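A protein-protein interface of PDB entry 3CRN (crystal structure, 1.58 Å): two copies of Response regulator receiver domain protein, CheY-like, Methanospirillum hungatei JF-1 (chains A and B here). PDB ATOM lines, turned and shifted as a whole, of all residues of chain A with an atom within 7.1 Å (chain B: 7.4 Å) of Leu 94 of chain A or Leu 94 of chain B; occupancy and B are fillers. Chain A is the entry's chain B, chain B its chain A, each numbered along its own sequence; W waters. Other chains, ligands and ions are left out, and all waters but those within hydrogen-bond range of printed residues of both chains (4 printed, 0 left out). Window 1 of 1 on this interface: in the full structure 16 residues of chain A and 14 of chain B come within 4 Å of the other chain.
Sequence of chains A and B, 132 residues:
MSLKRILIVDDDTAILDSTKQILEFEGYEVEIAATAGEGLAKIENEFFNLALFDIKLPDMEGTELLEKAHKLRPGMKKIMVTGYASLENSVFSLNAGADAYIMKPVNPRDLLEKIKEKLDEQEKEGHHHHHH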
ATOM      1  N   LEU A  66      26.291 -16.015 -17.447  1.00  0.00           N
ATOM      2  CA  LEU A  66      25.931 -17.351 -16.982  1.00  0.00           C
ATOM      3  C   LEU A  66      24.539 -17.770 -17.492  1.00  0.00           C
ATOM      4  O   LEU A  66      24.336 -18.862 -17.999  1.00  0.00           O
ATOM      5  CB  LEU A  66      25.922 -17.350 -15.461  1.00  0.00           C
ATOM      6  CG  LEU A  66      25.252 -18.574 -14.830  1.00  0.00           C
ATOM      7  CD1 LEU A  66      26.023 -19.863 -15.058  1.00  0.00           C
ATOM      8  CD2 LEU A  66      24.981 -18.295 -13.337  1.00  0.00           C
ATOM      9  N   LYS A  78      29.653 -24.770 -14.805  1.00  0.00           N
ATOM     10  CA  LYS A  78      29.940 -23.332 -14.661  1.00  0.00           C
ATOM     11  C   LYS A  78      30.314 -22.991 -13.227  1.00  0.00           C
ATOM     12  O   LYS A  78      29.552 -23.290 -12.306  1.00  0.00           O
ATOM     13  CB  LYS A  78      28.729 -22.474 -15.075  1.00  0.00           C
ATOM     14  CG  LYS A  78      28.239 -22.708 -16.528  1.00  0.00           C
ATOM     15  CD  LYS A  78      27.000 -23.614 -16.585  1.00  0.00           C
ATOM     16  CE  LYS A  78      26.548 -23.870 -18.032  1.00  0.00           C
ATOM     17  NZ  LYS A  78      25.479 -24.897 -18.036  1.00  0.00           N
ATOM     18  N   ILE A  79      31.497 -22.408 -13.046  1.00  0.00           N
ATOM     19  CA  ILE A  79      31.927 -22.019 -11.707  1.00  0.00           C
ATOM     20  C   ILE A  79      32.087 -20.513 -11.716  1.00  0.00           C
ATOM     21  O   ILE A  79      32.825 -19.982 -12.567  1.00  0.00           O
ATOM     22  CB  ILE A  79      33.290 -22.679 -11.369  1.00  0.00           C
ATOM     23  CG1 ILE A  79      33.184 -24.197 -11.465  1.00  0.00           C
ATOM     24  CG2 ILE A  79      33.764 -22.236  -9.955  1.00  0.00           C
ATOM     25  CD1 ILE A  79      34.465 -24.895 -11.014  1.00  0.00           C
ATOM     26  N   MET A  80      31.391 -19.820 -10.817  1.00  0.00           N
ATOM     27  CA  MET A  80      31.592 -18.371 -10.657  1.00  0.00           C
ATOM     28  C   MET A  80      32.837 -18.155  -9.822  1.00  0.00           C
ATOM     29  O   MET A  80      33.021 -18.813  -8.808  1.00  0.00           O
ATOM     30  CB  MET A  80      30.410 -17.678  -9.971  1.00  0.00           C
ATOM     31  CG  MET A  80      29.033 -18.148 -10.507  1.00  0.00           C
ATOM     32  SD  MET A  80      28.925 -18.020 -12.469  1.00  0.00           S
ATOM     33  CE  MET A  80      28.981 -16.050 -12.600  1.00  0.00           C
ATOM     34  N   GLU A  88      22.672 -10.919  -3.652  1.00  0.00           N
ATOM     35  CA  GLU A  88      21.942 -10.799  -4.910  1.00  0.00           C
ATOM     36  C   GLU A  88      22.573 -11.630  -6.036  1.00  0.00           C
ATOM     37  O   GLU A  88      21.897 -12.425  -6.690  1.00  0.00           O
ATOM     38  CB  GLU A  88      21.841  -9.312  -5.288  1.00  0.00           C
ATOM     39  CG  GLU A  88      21.587  -8.996  -6.756  1.00  0.00           C
ATOM     40  CD  GLU A  88      21.856  -7.519  -7.082  1.00  0.00           C
ATOM     41  OE1 GLU A  88      21.088  -6.647  -6.613  1.00  0.00           O
ATOM     42  OE2 GLU A  88      22.839  -7.230  -7.803  1.00  0.00           O
ATOM     43  N   ASN A  89      23.872 -11.475  -6.269  1.00  0.00           N
ATOM     44  CA  ASN A  89      24.472 -12.199  -7.387  1.00  0.00           C
ATOM     45  C   ASN A  89      24.739 -13.688  -7.112  1.00  0.00           C
ATOM     46  O   ASN A  89      24.848 -14.478  -8.045  1.00  0.00           O
ATOM     47  CB  ASN A  89      25.682 -11.456  -8.011  1.00  0.00           C
ATOM     48  CG  ASN A  89      26.896 -11.386  -7.083  1.00  0.00           C
ATOM     49  OD1 ASN A  89      27.162 -12.302  -6.302  1.00  0.00           O
ATOM     50  ND2 ASN A  89      27.657 -10.297  -7.201  1.00  0.00           N
ATOM     51  N   SER A  90      24.811 -14.069  -5.835  1.00  0.00           N
ATOM     52  CA  SER A  90      24.954 -15.491  -5.495  1.00  0.00           C
ATOM     53  C   SER A  90      23.626 -16.216  -5.657  1.00  0.00           C
ATOM     54  O   SER A  90      23.567 -17.311  -6.254  1.00  0.00           O
ATOM     55  CB  SER A  90      25.533 -15.692  -4.086  1.00  0.00           C
ATOM     56  OG  SER A  90      24.703 -15.160  -3.074  1.00  0.00           O
ATOM     57  N   VAL A  91      22.551 -15.614  -5.158  1.00  0.00           N
ATOM     58  CA  VAL A  91      21.221 -16.206  -5.384  1.00  0.00           C
ATOM     59  C   VAL A  91      20.925 -16.288  -6.892  1.00  0.00           C
ATOM     60  O   VAL A  91      20.454 -17.315  -7.395  1.00  0.00           O
ATOM     61  CB  VAL A  91      20.093 -15.453  -4.596  1.00  0.00           C
ATOM     62  CG1 VAL A  91      18.706 -15.896  -5.084  1.00  0.00           C
ATOM     63  CG2 VAL A  91      20.234 -15.692  -3.096  1.00  0.00           C
ATOM     64  N   PHE A  92      21.244 -15.231  -7.631  1.00  0.00           N
ATOM     65  CA  PHE A  92      21.016 -15.240  -9.073  1.00  0.00           C
ATOM     66  C   PHE A  92      21.820 -16.339  -9.746  1.00  0.00           C
ATOM     67  O   PHE A  92      21.296 -17.073 -10.591  1.00  0.00           O
ATOM     68  CB  PHE A  92      21.375 -13.888  -9.717  1.00  0.00           C
ATOM     69  CG  PHE A  92      20.936 -13.776 -11.168  1.00  0.00           C
ATOM     70  CD1 PHE A  92      19.772 -13.100 -11.509  1.00  0.00           C
ATOM     71  CD2 PHE A  92      21.676 -14.363 -12.187  1.00  0.00           C
ATOM     72  CE1 PHE A  92      19.371 -13.002 -12.840  1.00  0.00           C
ATOM     73  CE2 PHE A  92      21.268 -14.266 -13.523  1.00  0.00           C
ATOM     74  CZ  PHE A  92      20.125 -13.586 -13.841  1.00  0.00           C
ATOM     75  N   SER A  93      23.104 -16.447  -9.388  1.00  0.00           N
ATOM     76  CA  SER A  93      23.973 -17.498  -9.949  1.00  0.00           C
ATOM     77  C   SER A  93      23.407 -18.891  -9.685  1.00  0.00           C
ATOM     78  O   SER A  93      23.426 -19.756 -10.565  1.00  0.00           O
ATOM     79  CB  SER A  93      25.384 -17.403  -9.336  1.00  0.00           C
ATOM     80  OG  SER A  93      26.004 -16.185  -9.747  1.00  0.00           O
ATOM     81  N   LEU A  94      22.932 -19.120  -8.451  1.00  0.00           N
ATOM     82  CA  LEU A  94      22.292 -20.400  -8.116  1.00  0.00           C
ATOM     83  C   LEU A  94      21.108 -20.677  -9.064  1.00  0.00           C
ATOM     84  O   LEU A  94      21.035 -21.720  -9.712  1.00  0.00           O
ATOM     85  CB  LEU A  94      21.793 -20.330  -6.682  1.00  0.00           C
ATOM     86  CG  LEU A  94      21.512 -21.671  -6.009  1.00  0.00           C
ATOM     87  CD1 LEU A  94      21.567 -21.507  -4.507  1.00  0.00           C
ATOM     88  CD2 LEU A  94      20.179 -22.242  -6.479  1.00  0.00           C
ATOM     89  N   ASN A  95      20.202 -19.712  -9.162  1.00  0.00           N
ATOM     90  CA  ASN A  95      18.992 -19.881 -10.003  1.00  0.00           C
ATOM     91  C   ASN A  95      19.288 -20.019 -11.496  1.00  0.00           C
ATOM     92  O   ASN A  95      18.583 -20.729 -12.227  1.00  0.00           O
ATOM     93  CB  ASN A  95      18.012 -18.741  -9.717  1.00  0.00           C
ATOM     94  CG  ASN A  95      17.328 -18.922  -8.364  1.00  0.00           C
ATOM     95  OD1 ASN A  95      17.016 -20.055  -7.985  1.00  0.00           O
ATOM     96  ND2 ASN A  95      17.085 -17.820  -7.645  1.00  0.00           N
ATOM     97  N   ALA A  96      20.378 -19.384 -11.919  1.00  0.00           N
ATOM     98  CA  ALA A  96      20.737 -19.329 -13.330  1.00  0.00           C
ATOM     99  C   ALA A  96      21.571 -20.518 -13.814  1.00  0.00           C
ATOM    100  O   ALA A  96      21.890 -20.604 -15.004  1.00  0.00           O
ATOM    101  CB  ALA A  96      21.463 -17.993 -13.644  1.00  0.00           C
ATOM    102  N   GLY A  97      21.933 -21.421 -12.900  1.00  0.00           N
ATOM    103  CA  GLY A  97      22.581 -22.673 -13.298  1.00  0.00           C
ATOM    104  C   GLY A  97      24.037 -22.915 -12.889  1.00  0.00           C
ATOM    105  O   GLY A  97      24.621 -23.909 -13.302  1.00  0.00           O
ATOM    106  N   ALA A  98      24.616 -22.025 -12.080  1.00  0.00           N
ATOM    107  CA  ALA A  98      26.021 -22.186 -11.670  1.00  0.00           C
ATOM    108  C   ALA A  98      26.187 -23.477 -10.898  1.00  0.00           C
ATOM    109  O   ALA A  98      25.299 -23.840 -10.138  1.00  0.00           O
ATOM    110  CB  ALA A  98      26.464 -21.039 -10.810  1.00  0.00           C
ATOM    111  N   ASP A  99      27.322 -24.165 -11.066  1.00  0.00           N
ATOM    112  CA  ASP A  99      27.563 -25.420 -10.370  1.00  0.00           C
ATOM    113  C   ASP A  99      28.411 -25.230  -9.123  1.00  0.00           C
ATOM    114  O   ASP A  99      28.407 -26.053  -8.212  1.00  0.00           O
ATOM    115  CB  ASP A  99      28.261 -26.409 -11.300  1.00  0.00           C
ATOM    116  CG  ASP A  99      27.364 -26.805 -12.443  1.00  0.00           C
ATOM    117  OD1 ASP A  99      26.440 -27.619 -12.218  1.00  0.00           O
ATOM    118  OD2 ASP A  99      27.540 -26.264 -13.541  1.00  0.00           O
ATOM    119  N   ALA A 100      29.173 -24.144  -9.117  1.00  0.00           N
ATOM    120  CA  ALA A 100      29.960 -23.778  -7.936  1.00  0.00           C
ATOM    121  C   ALA A 100      30.228 -22.289  -7.937  1.00  0.00           C
ATOM    122  O   ALA A 100      30.061 -21.612  -8.952  1.00  0.00           O
ATOM    123  CB  ALA A 100      31.270 -24.537  -7.896  1.00  0.00           C
ATOM    124  N   TYR A 101      30.674 -21.788  -6.790  1.00  0.00           N
ATOM    125  CA  TYR A 101      30.796 -20.353  -6.584  1.00  0.00           C
ATOM    126  C   TYR A 101      31.961 -20.147  -5.635  1.00  0.00           C
ATOM    127  O   TYR A 101      31.917 -20.609  -4.498  1.00  0.00           O
ATOM    128  CB  TYR A 101      29.489 -19.805  -6.015  1.00  0.00           C
ATOM    129  CG  TYR A 101      29.405 -18.296  -5.914  1.00  0.00           C
ATOM    130  CD1 TYR A 101      28.569 -17.577  -6.760  1.00  0.00           C
ATOM    131  CD2 TYR A 101      30.132 -17.593  -4.942  1.00  0.00           C
ATOM    132  CE1 TYR A 101      28.454 -16.204  -6.654  1.00  0.00           C
ATOM    133  CE2 TYR A 101      30.018 -16.194  -4.827  1.00  0.00           C
ATOM    134  CZ  TYR A 101      29.190 -15.515  -5.700  1.00  0.00           C
ATOM    135  OH  TYR A 101      29.078 -14.142  -5.635  1.00  0.00           O
ATOM    136  N   ILE A 102      32.986 -19.464  -6.129  1.00  0.00           N
ATOM    137  CA  ILE A 102      34.249 -19.310  -5.406  1.00  0.00           C
ATOM    138  C   ILE A 102      34.558 -17.829  -5.249  1.00  0.00           C
ATOM    139  O   ILE A 102      34.433 -17.066  -6.207  1.00  0.00           O
ATOM    140  CB  ILE A 102      35.420 -19.931  -6.194  1.00  0.00           C
ATOM    141  CG1 ILE A 102      35.267 -21.445  -6.326  1.00  0.00           C
ATOM    142  CG2 ILE A 102      36.756 -19.599  -5.528  1.00  0.00           C
ATOM    143  CD1 ILE A 102      36.325 -22.076  -7.229  1.00  0.00           C
ATOM    144  N   LYS A 118      33.845 -31.084 -10.476  1.00  0.00           N
ATOM    145  CA  LYS A 118      32.734 -30.791 -11.381  1.00  0.00           C
ATOM    146  C   LYS A 118      32.875 -31.588 -12.694  1.00  0.00           C
ATOM    147  O   LYS A 118      31.888 -32.004 -13.305  1.00  0.00           O
ATOM    148  CB  LYS A 118      32.609 -29.277 -11.651  1.00  0.00           C
ATOM    149  CG  LYS A 118      32.323 -28.410 -10.416  1.00  0.00           C
ATOM    150  CD  LYS A 118      31.068 -28.917  -9.694  1.00  0.00           C
ATOM    151  CE  LYS A 118      31.343 -29.063  -8.213  1.00  0.00           C
ATOM    152  NZ  LYS A 118      30.147 -29.552  -7.488  1.00  0.00           N
ATOM    153  N   LEU B  66      19.987 -29.776   3.600  1.00  0.00           N
ATOM    154  CA  LEU B  66      20.259 -29.886   2.152  1.00  0.00           C
ATOM    155  C   LEU B  66      21.363 -30.931   1.884  1.00  0.00           C
ATOM    156  O   LEU B  66      21.191 -31.857   1.073  1.00  0.00           O
ATOM    157  CB  LEU B  66      20.683 -28.532   1.610  1.00  0.00           C
ATOM    158  CG  LEU B  66      21.264 -28.553   0.191  1.00  0.00           C
ATOM    159  CD1 LEU B  66      20.264 -29.063  -0.862  1.00  0.00           C
ATOM    160  CD2 LEU B  66      21.853 -27.157  -0.204  1.00  0.00           C
ATOM    161  N   LYS B  78      16.050 -29.786  -5.299  1.00  0.00           N
ATOM    162  CA  LYS B  78      15.952 -29.116  -4.001  1.00  0.00           C
ATOM    163  C   LYS B  78      15.867 -27.605  -4.195  1.00  0.00           C
ATOM    164  O   LYS B  78      16.721 -27.038  -4.875  1.00  0.00           O
ATOM    165  CB  LYS B  78      17.179 -29.447  -3.135  1.00  0.00           C
ATOM    166  CG  LYS B  78      17.300 -30.950  -2.827  1.00  0.00           C
ATOM    167  CD  LYS B  78      18.500 -31.585  -3.538  1.00  0.00           C
ATOM    168  CE  LYS B  78      18.600 -33.106  -3.274  1.00  0.00           C
ATOM    169  NZ  LYS B  78      19.434 -33.674  -4.371  1.00  0.00           N
ATOM    170  N   ILE B  79      14.839 -26.962  -3.636  1.00  0.00           N
ATOM    171  CA  ILE B  79      14.733 -25.523  -3.742  1.00  0.00           C
ATOM    172  C   ILE B  79      14.704 -24.952  -2.336  1.00  0.00           C
ATOM    173  O   ILE B  79      13.897 -25.403  -1.532  1.00  0.00           O
ATOM    174  CB  ILE B  79      13.411 -25.139  -4.455  1.00  0.00           C
ATOM    175  CG1 ILE B  79      13.408 -25.769  -5.863  1.00  0.00           C
ATOM    176  CG2 ILE B  79      13.248 -23.602  -4.491  1.00  0.00           C
ATOM    177  CD1 ILE B  79      12.226 -25.320  -6.764  1.00  0.00           C
ATOM    178  N   MET B  80      15.609 -24.017  -2.019  1.00  0.00           N
ATOM    179  CA  MET B  80      15.623 -23.383  -0.683  1.00  0.00           C
ATOM    180  C   MET B  80      14.544 -22.303  -0.726  1.00  0.00           C
ATOM    181  O   MET B  80      14.404 -21.600  -1.734  1.00  0.00           O
ATOM    182  CB  MET B  80      17.003 -22.757  -0.420  1.00  0.00           C
ATOM    183  CG  MET B  80      18.202 -23.638  -0.742  1.00  0.00           C
ATOM    184  SD  MET B  80      18.010 -25.434   0.081  1.00  0.00           S
ATOM    185  CE  MET B  80      18.253 -24.838   1.948  1.00  0.00           C
ATOM    186  N   GLU B  88      26.352 -15.997   2.976  1.00  0.00           N
ATOM    187  CA  GLU B  88      26.888 -17.269   3.441  1.00  0.00           C
ATOM    188  C   GLU B  88      25.998 -18.471   3.092  1.00  0.00           C
ATOM    189  O   GLU B  88      26.492 -19.486   2.552  1.00  0.00           O
ATOM    190  CB  GLU B  88      27.106 -17.215   4.949  1.00  0.00           C
ATOM    191  CG  GLU B  88      27.372 -18.566   5.573  1.00  0.00           C
ATOM    192  CD  GLU B  88      28.120 -18.454   6.888  1.00  0.00           C
ATOM    193  OE1 GLU B  88      29.225 -17.872   6.895  1.00  0.00           O
ATOM    194  OE2 GLU B  88      27.605 -18.954   7.908  1.00  0.00           O
ATOM    195  N   ASN B  89      24.703 -18.383   3.404  1.00  0.00           N
ATOM    196  CA  ASN B  89      23.850 -19.568   3.179  1.00  0.00           C
ATOM    197  C   ASN B  89      23.414 -19.756   1.715  1.00  0.00           C
ATOM    198  O   ASN B  89      23.139 -20.884   1.301  1.00  0.00           O
ATOM    199  CB  ASN B  89      22.687 -19.731   4.189  1.00  0.00           C
ATOM    200  CG  ASN B  89      21.629 -18.634   4.095  1.00  0.00           C
ATOM    201  OD1 ASN B  89      21.335 -18.105   3.018  1.00  0.00           O
ATOM    202  ND2 ASN B  89      21.016 -18.310   5.252  1.00  0.00           N
ATOM    203  N   SER B  90      23.425 -18.684   0.929  1.00  0.00           N
ATOM    204  CA  SER B  90      23.150 -18.821  -0.503  1.00  0.00           C
ATOM    205  C   SER B  90      24.356 -19.450  -1.207  1.00  0.00           C
ATOM    206  O   SER B  90      24.189 -20.394  -1.985  1.00  0.00           O
ATOM    207  CB  SER B  90      22.799 -17.495  -1.171  1.00  0.00           C
ATOM    208  OG  SER B  90      23.809 -16.532  -0.953  1.00  0.00           O
ATOM    209  N   VAL B  91      25.568 -18.948  -0.917  1.00  0.00           N
ATOM    210  CA  VAL B  91      26.783 -19.574  -1.488  1.00  0.00           C
ATOM    211  C   VAL B  91      26.896 -21.037  -1.070  1.00  0.00           C
ATOM    212  O   VAL B  91      27.178 -21.915  -1.901  1.00  0.00           O
ATOM    213  CB  VAL B  91      28.060 -18.786  -1.102  1.00  0.00           C
ATOM    214  CG1 VAL B  91      29.323 -19.564  -1.467  1.00  0.00           C
ATOM    215  CG2 VAL B  91      28.018 -17.416  -1.767  1.00  0.00           C
ATOM    216  N   PHE B  92      26.653 -21.309   0.211  1.00  0.00           N
ATOM    217  CA  PHE B  92      26.673 -22.697   0.681  1.00  0.00           C
ATOM    218  C   PHE B  92      25.655 -23.558  -0.088  1.00  0.00           C
ATOM    219  O   PHE B  92      25.976 -24.651  -0.569  1.00  0.00           O
ATOM    220  CB  PHE B  92      26.341 -22.786   2.165  1.00  0.00           C
ATOM    221  CG  PHE B  92      26.465 -24.163   2.697  1.00  0.00           C
ATOM    222  CD1 PHE B  92      27.635 -24.573   3.336  1.00  0.00           C
ATOM    223  CD2 PHE B  92      25.446 -25.076   2.514  1.00  0.00           C
ATOM    224  CE1 PHE B  92      27.768 -25.870   3.821  1.00  0.00           C
ATOM    225  CE2 PHE B  92      25.570 -26.390   2.996  1.00  0.00           C
ATOM    226  CZ  PHE B  92      26.740 -26.777   3.653  1.00  0.00           C
ATOM    227  N   SER B  93      24.428 -23.064  -0.209  1.00  0.00           N
ATOM    228  CA  SER B  93      23.392 -23.846  -0.884  1.00  0.00           C
ATOM    229  C   SER B  93      23.766 -24.090  -2.348  1.00  0.00           C
ATOM    230  O   SER B  93      23.524 -25.169  -2.884  1.00  0.00           O
ATOM    231  CB  SER B  93      22.046 -23.135  -0.765  1.00  0.00           C
ATOM    232  OG  SER B  93      21.682 -23.038   0.600  1.00  0.00           O
ATOM    233  N   LEU B  94      24.328 -23.075  -3.000  1.00  0.00           N
ATOM    234  CA  LEU B  94      24.760 -23.247  -4.395  1.00  0.00           C
ATOM    235  C   LEU B  94      25.805 -24.377  -4.494  1.00  0.00           C
ATOM    236  O   LEU B  94      25.691 -25.305  -5.301  1.00  0.00           O
ATOM    237  CB  LEU B  94      25.365 -21.936  -4.903  1.00  0.00           C
ATOM    238  CG  LEU B  94      25.650 -21.717  -6.385  1.00  0.00           C
ATOM    239  CD1 LEU B  94      25.885 -20.240  -6.628  1.00  0.00           C
ATOM    240  CD2 LEU B  94      26.832 -22.555  -6.834  1.00  0.00           C
ATOM    241  N   ASN B  95      26.850 -24.273  -3.670  1.00  0.00           N
ATOM    242  CA  ASN B  95      27.925 -25.246  -3.715  1.00  0.00           C
ATOM    243  C   ASN B  95      27.490 -26.647  -3.279  1.00  0.00           C
ATOM    244  O   ASN B  95      28.073 -27.650  -3.727  1.00  0.00           O
ATOM    245  CB  ASN B  95      29.109 -24.743  -2.872  1.00  0.00           C
ATOM    246  CG  ASN B  95      29.856 -23.611  -3.561  1.00  0.00           C
ATOM    247  OD1 ASN B  95      30.082 -23.664  -4.777  1.00  0.00           O
ATOM    248  ND2 ASN B  95      30.248 -22.589  -2.802  1.00  0.00           N
ATOM    249  N   ALA B  96      26.461 -26.720  -2.433  1.00  0.00           N
ATOM    250  CA  ALA B  96      26.019 -27.999  -1.877  1.00  0.00           C
ATOM    251  C   ALA B  96      24.973 -28.669  -2.756  1.00  0.00           C
ATOM    252  O   ALA B  96      24.511 -29.757  -2.437  1.00  0.00           O
ATOM    253  CB  ALA B  96      25.504 -27.837  -0.456  1.00  0.00           C
ATOM    254  N   GLY B  97      24.600 -28.004  -3.849  1.00  0.00           N
ATOM    255  CA  GLY B  97      23.778 -28.651  -4.872  1.00  0.00           C
ATOM    256  C   GLY B  97      22.309 -28.236  -4.979  1.00  0.00           C
ATOM    257  O   GLY B  97      21.543 -28.885  -5.698  1.00  0.00           O
ATOM    258  N   ALA B  98      21.904 -27.180  -4.276  1.00  0.00           N
ATOM    259  CA  ALA B  98      20.524 -26.685  -4.401  1.00  0.00           C
ATOM    260  C   ALA B  98      20.225 -26.348  -5.857  1.00  0.00           C
ATOM    261  O   ALA B  98      21.099 -25.934  -6.601  1.00  0.00           O
ATOM    262  CB  ALA B  98      20.306 -25.454  -3.529  1.00  0.00           C
ATOM    263  N   ASP B  99      18.981 -26.547  -6.279  1.00  0.00           N
ATOM    264  CA  ASP B  99      18.619 -26.291  -7.661  1.00  0.00           C
ATOM    265  C   ASP B  99      18.007 -24.912  -7.910  1.00  0.00           C
ATOM    266  O   ASP B  99      17.993 -24.420  -9.047  1.00  0.00           O
ATOM    267  CB  ASP B  99      17.676 -27.389  -8.109  1.00  0.00           C
ATOM    268  CG  ASP B  99      18.367 -28.737  -8.090  1.00  0.00           C
ATOM    269  OD1 ASP B  99      19.286 -28.921  -8.923  1.00  0.00           O
ATOM    270  OD2 ASP B  99      18.051 -29.579  -7.210  1.00  0.00           O
ATOM    271  N   ALA B 100      17.438 -24.325  -6.857  1.00  0.00           N
ATOM    272  CA  ALA B 100      16.908 -22.979  -6.933  1.00  0.00           C
ATOM    273  C   ALA B 100      16.793 -22.447  -5.524  1.00  0.00           C
ATOM    274  O   ALA B 100      16.954 -23.192  -4.566  1.00  0.00           O
ATOM    275  CB  ALA B 100      15.535 -22.976  -7.622  1.00  0.00           C
ATOM    276  N   TYR B 101      16.500 -21.161  -5.406  1.00  0.00           N
ATOM    277  CA  TYR B 101      16.578 -20.495  -4.121  1.00  0.00           C
ATOM    278  C   TYR B 101      15.646 -19.307  -4.199  1.00  0.00           C
ATOM    279  O   TYR B 101      15.774 -18.466  -5.080  1.00  0.00           O
ATOM    280  CB  TYR B 101      18.023 -20.062  -3.897  1.00  0.00           C
ATOM    281  CG  TYR B 101      18.324 -19.473  -2.541  1.00  0.00           C
ATOM    282  CD1 TYR B 101      19.176 -20.122  -1.656  1.00  0.00           C
ATOM    283  CD2 TYR B 101      17.765 -18.258  -2.135  1.00  0.00           C
ATOM    284  CE1 TYR B 101      19.488 -19.551  -0.412  1.00  0.00           C
ATOM    285  CE2 TYR B 101      18.053 -17.702  -0.889  1.00  0.00           C
ATOM    286  CZ  TYR B 101      18.896 -18.361  -0.028  1.00  0.00           C
ATOM    287  OH  TYR B 101      19.194 -17.809   1.217  1.00  0.00           O
ATOM    288  N   ILE B 102      14.665 -19.287  -3.302  1.00  0.00           N
ATOM    289  CA  ILE B 102      13.608 -18.269  -3.342  1.00  0.00           C
ATOM    290  C   ILE B 102      13.532 -17.542  -2.015  1.00  0.00           C
ATOM    291  O   ILE B 102      13.481 -18.180  -0.968  1.00  0.00           O
ATOM    292  CB  ILE B 102      12.242 -18.927  -3.592  1.00  0.00           C
ATOM    293  CG1 ILE B 102      12.183 -19.637  -4.955  1.00  0.00           C
ATOM    294  CG2 ILE B 102      11.124 -17.871  -3.560  1.00  0.00           C
ATOM    295  CD1 ILE B 102      10.830 -20.345  -5.180  1.00  0.00           C
ATOM    296  N   LYS B 118      12.365 -27.082 -12.787  1.00  0.00           N
ATOM    297  CA  LYS B 118      13.267 -28.066 -12.204  1.00  0.00           C
ATOM    298  C   LYS B 118      12.800 -29.507 -12.529  1.00  0.00           C
ATOM    299  O   LYS B 118      13.634 -30.401 -12.733  1.00  0.00           O
ATOM    300  CB  LYS B 118      13.473 -27.847 -10.704  1.00  0.00           C
ATOM    301  CG  LYS B 118      14.111 -26.507 -10.310  1.00  0.00           C
ATOM    302  CD  LYS B 118      15.329 -26.146 -11.122  1.00  0.00           C
ATOM    303  CE  LYS B 118      15.027 -25.038 -12.114  1.00  0.00           C
ATOM    304  NZ  LYS B 118      16.215 -24.632 -12.923  1.00  0.00           N
HETATM  305  O   HOH W   1      26.533 -27.670  -7.290  1.00  0.00           O
HETATM  306  O   HOH W   2      29.618 -27.351  -5.918  1.00  0.00           O
HETATM  307  O   HOH W   3      17.025 -22.770 -10.977  1.00  0.00           O
HETATM  308  O   HOH W   4      18.696 -23.033 -13.924  1.00  0.00           O
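CD1 of Leu 94 of chain B touches O of Ser 90 of chain A (3.8 Å).
CG2 of Val 91 of chain A touches CD2 of Tyr 101 of chain B, 3.7 Å away.
Leu 94 of chain A touches Ala 98 of chain B.
CB of Tyr 101 of chain B touches CD1 of Leu 94 of chain A, 3.9 Å away.
CG2 of Val 91 of chain B touches CD2 of Tyr 101 of chain A, 3.8 Å away.
Tyr 101 of chain A touches Leu 94 of chain B (CB to CD1, 3.7 Å).
Val 91 of chain A touches Tyr 101 of chain B, and with the chains exchanged Tyr 101 of chain A touches Val 91 of chain B.
Leu 94 of chain A touches Ala 98 of chain B, and with the chains exchanged Ala 98 of chain A touches Leu 94 of chain B.
Leu 94 of chain A touches Tyr 101 of chain B, and with the chains exchanged Tyr 101 of chain A touches Leu 94 of chain B.
Phe 92 of chain A touches none of the printed residues of chain B.
Of chain B, only Ser 90 (3.8 Å), Leu 94 (3.5 Å), Ala 98 (3.8 Å), Asp 99 (3.7 Å), Ala 100 (3.4 Å) and Tyr 101 (3.9 Å) come within 4 Å of Leu 94 of chain A.
Of the printed residues of chain B, Asp 99 of chain A touches Leu 94.
Of the printed residues of chain A, Ser 90 of chain B touches Ser 90, Val 91 and Leu 94.
Printed residues of chain A within 4 Å of Asn 95 of chain B: Ala 100 (3.2 Å) and Tyr 101 (2.8 Å).
The backbone carbonyl oxygen (O) of Lys 78 of chain B is in hydrogen-bond range of the backbone NH (N) of Ala 100 of chain B (3.4 Å).
The backbone carbonyl oxygen (O) of Ser 93 of chain A sits at hydrogen-bond distance from the backbone NH (N) of Ala 98 of chain A.
OG of Ser 90 of chain B sits at hydrogen-bond distance from OG of Ser 90 of chain A (2.7 Å).
The side-chain amide oxygen (OD1) of Asn 95 of chain B lies within hydrogen-bond range of the backbone NH (N) of Tyr 101 of chain A, 2.8 Å away.
The backbone NH (N) of Tyr 101 of chain B lies within hydrogen-bond range of the side-chain amide oxygen (OD1) of Asn 95 of chain A, at 2.9 Å.
Hydrophobic or aromatic side chains of chain A within 4 Å of the printed part of chain B: Val 91, Leu 94, Ala 100 and Tyr 101.
Of the 20 printed residues of chain B, 8 touch a printed residue of chain A.
Hydrophobic or aromatic side chains of chain B within 4 Å of the printed part of chain A: Val 91, Leu 94, Ala 100 and Tyr 101.
Among the printed residues, no Asp or Glu carboxylate lies within 4 Å of a Lys or Arg side-chain nitrogen of the other chain.
Water W1 lies within hydrogen-bond range of the backbone carbonyl oxygen (O) of Asp 99 of chain A and the backbone carbonyl oxygen (O) of Leu 94 of chain B.
Water W3 lies within hydrogen-bond range of O of Asp 99 of chain B (2.7 Å), NZ of Lys 118 of chain B (2.8 Å) and O of Asn 95 of chain A (2.9 Å).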
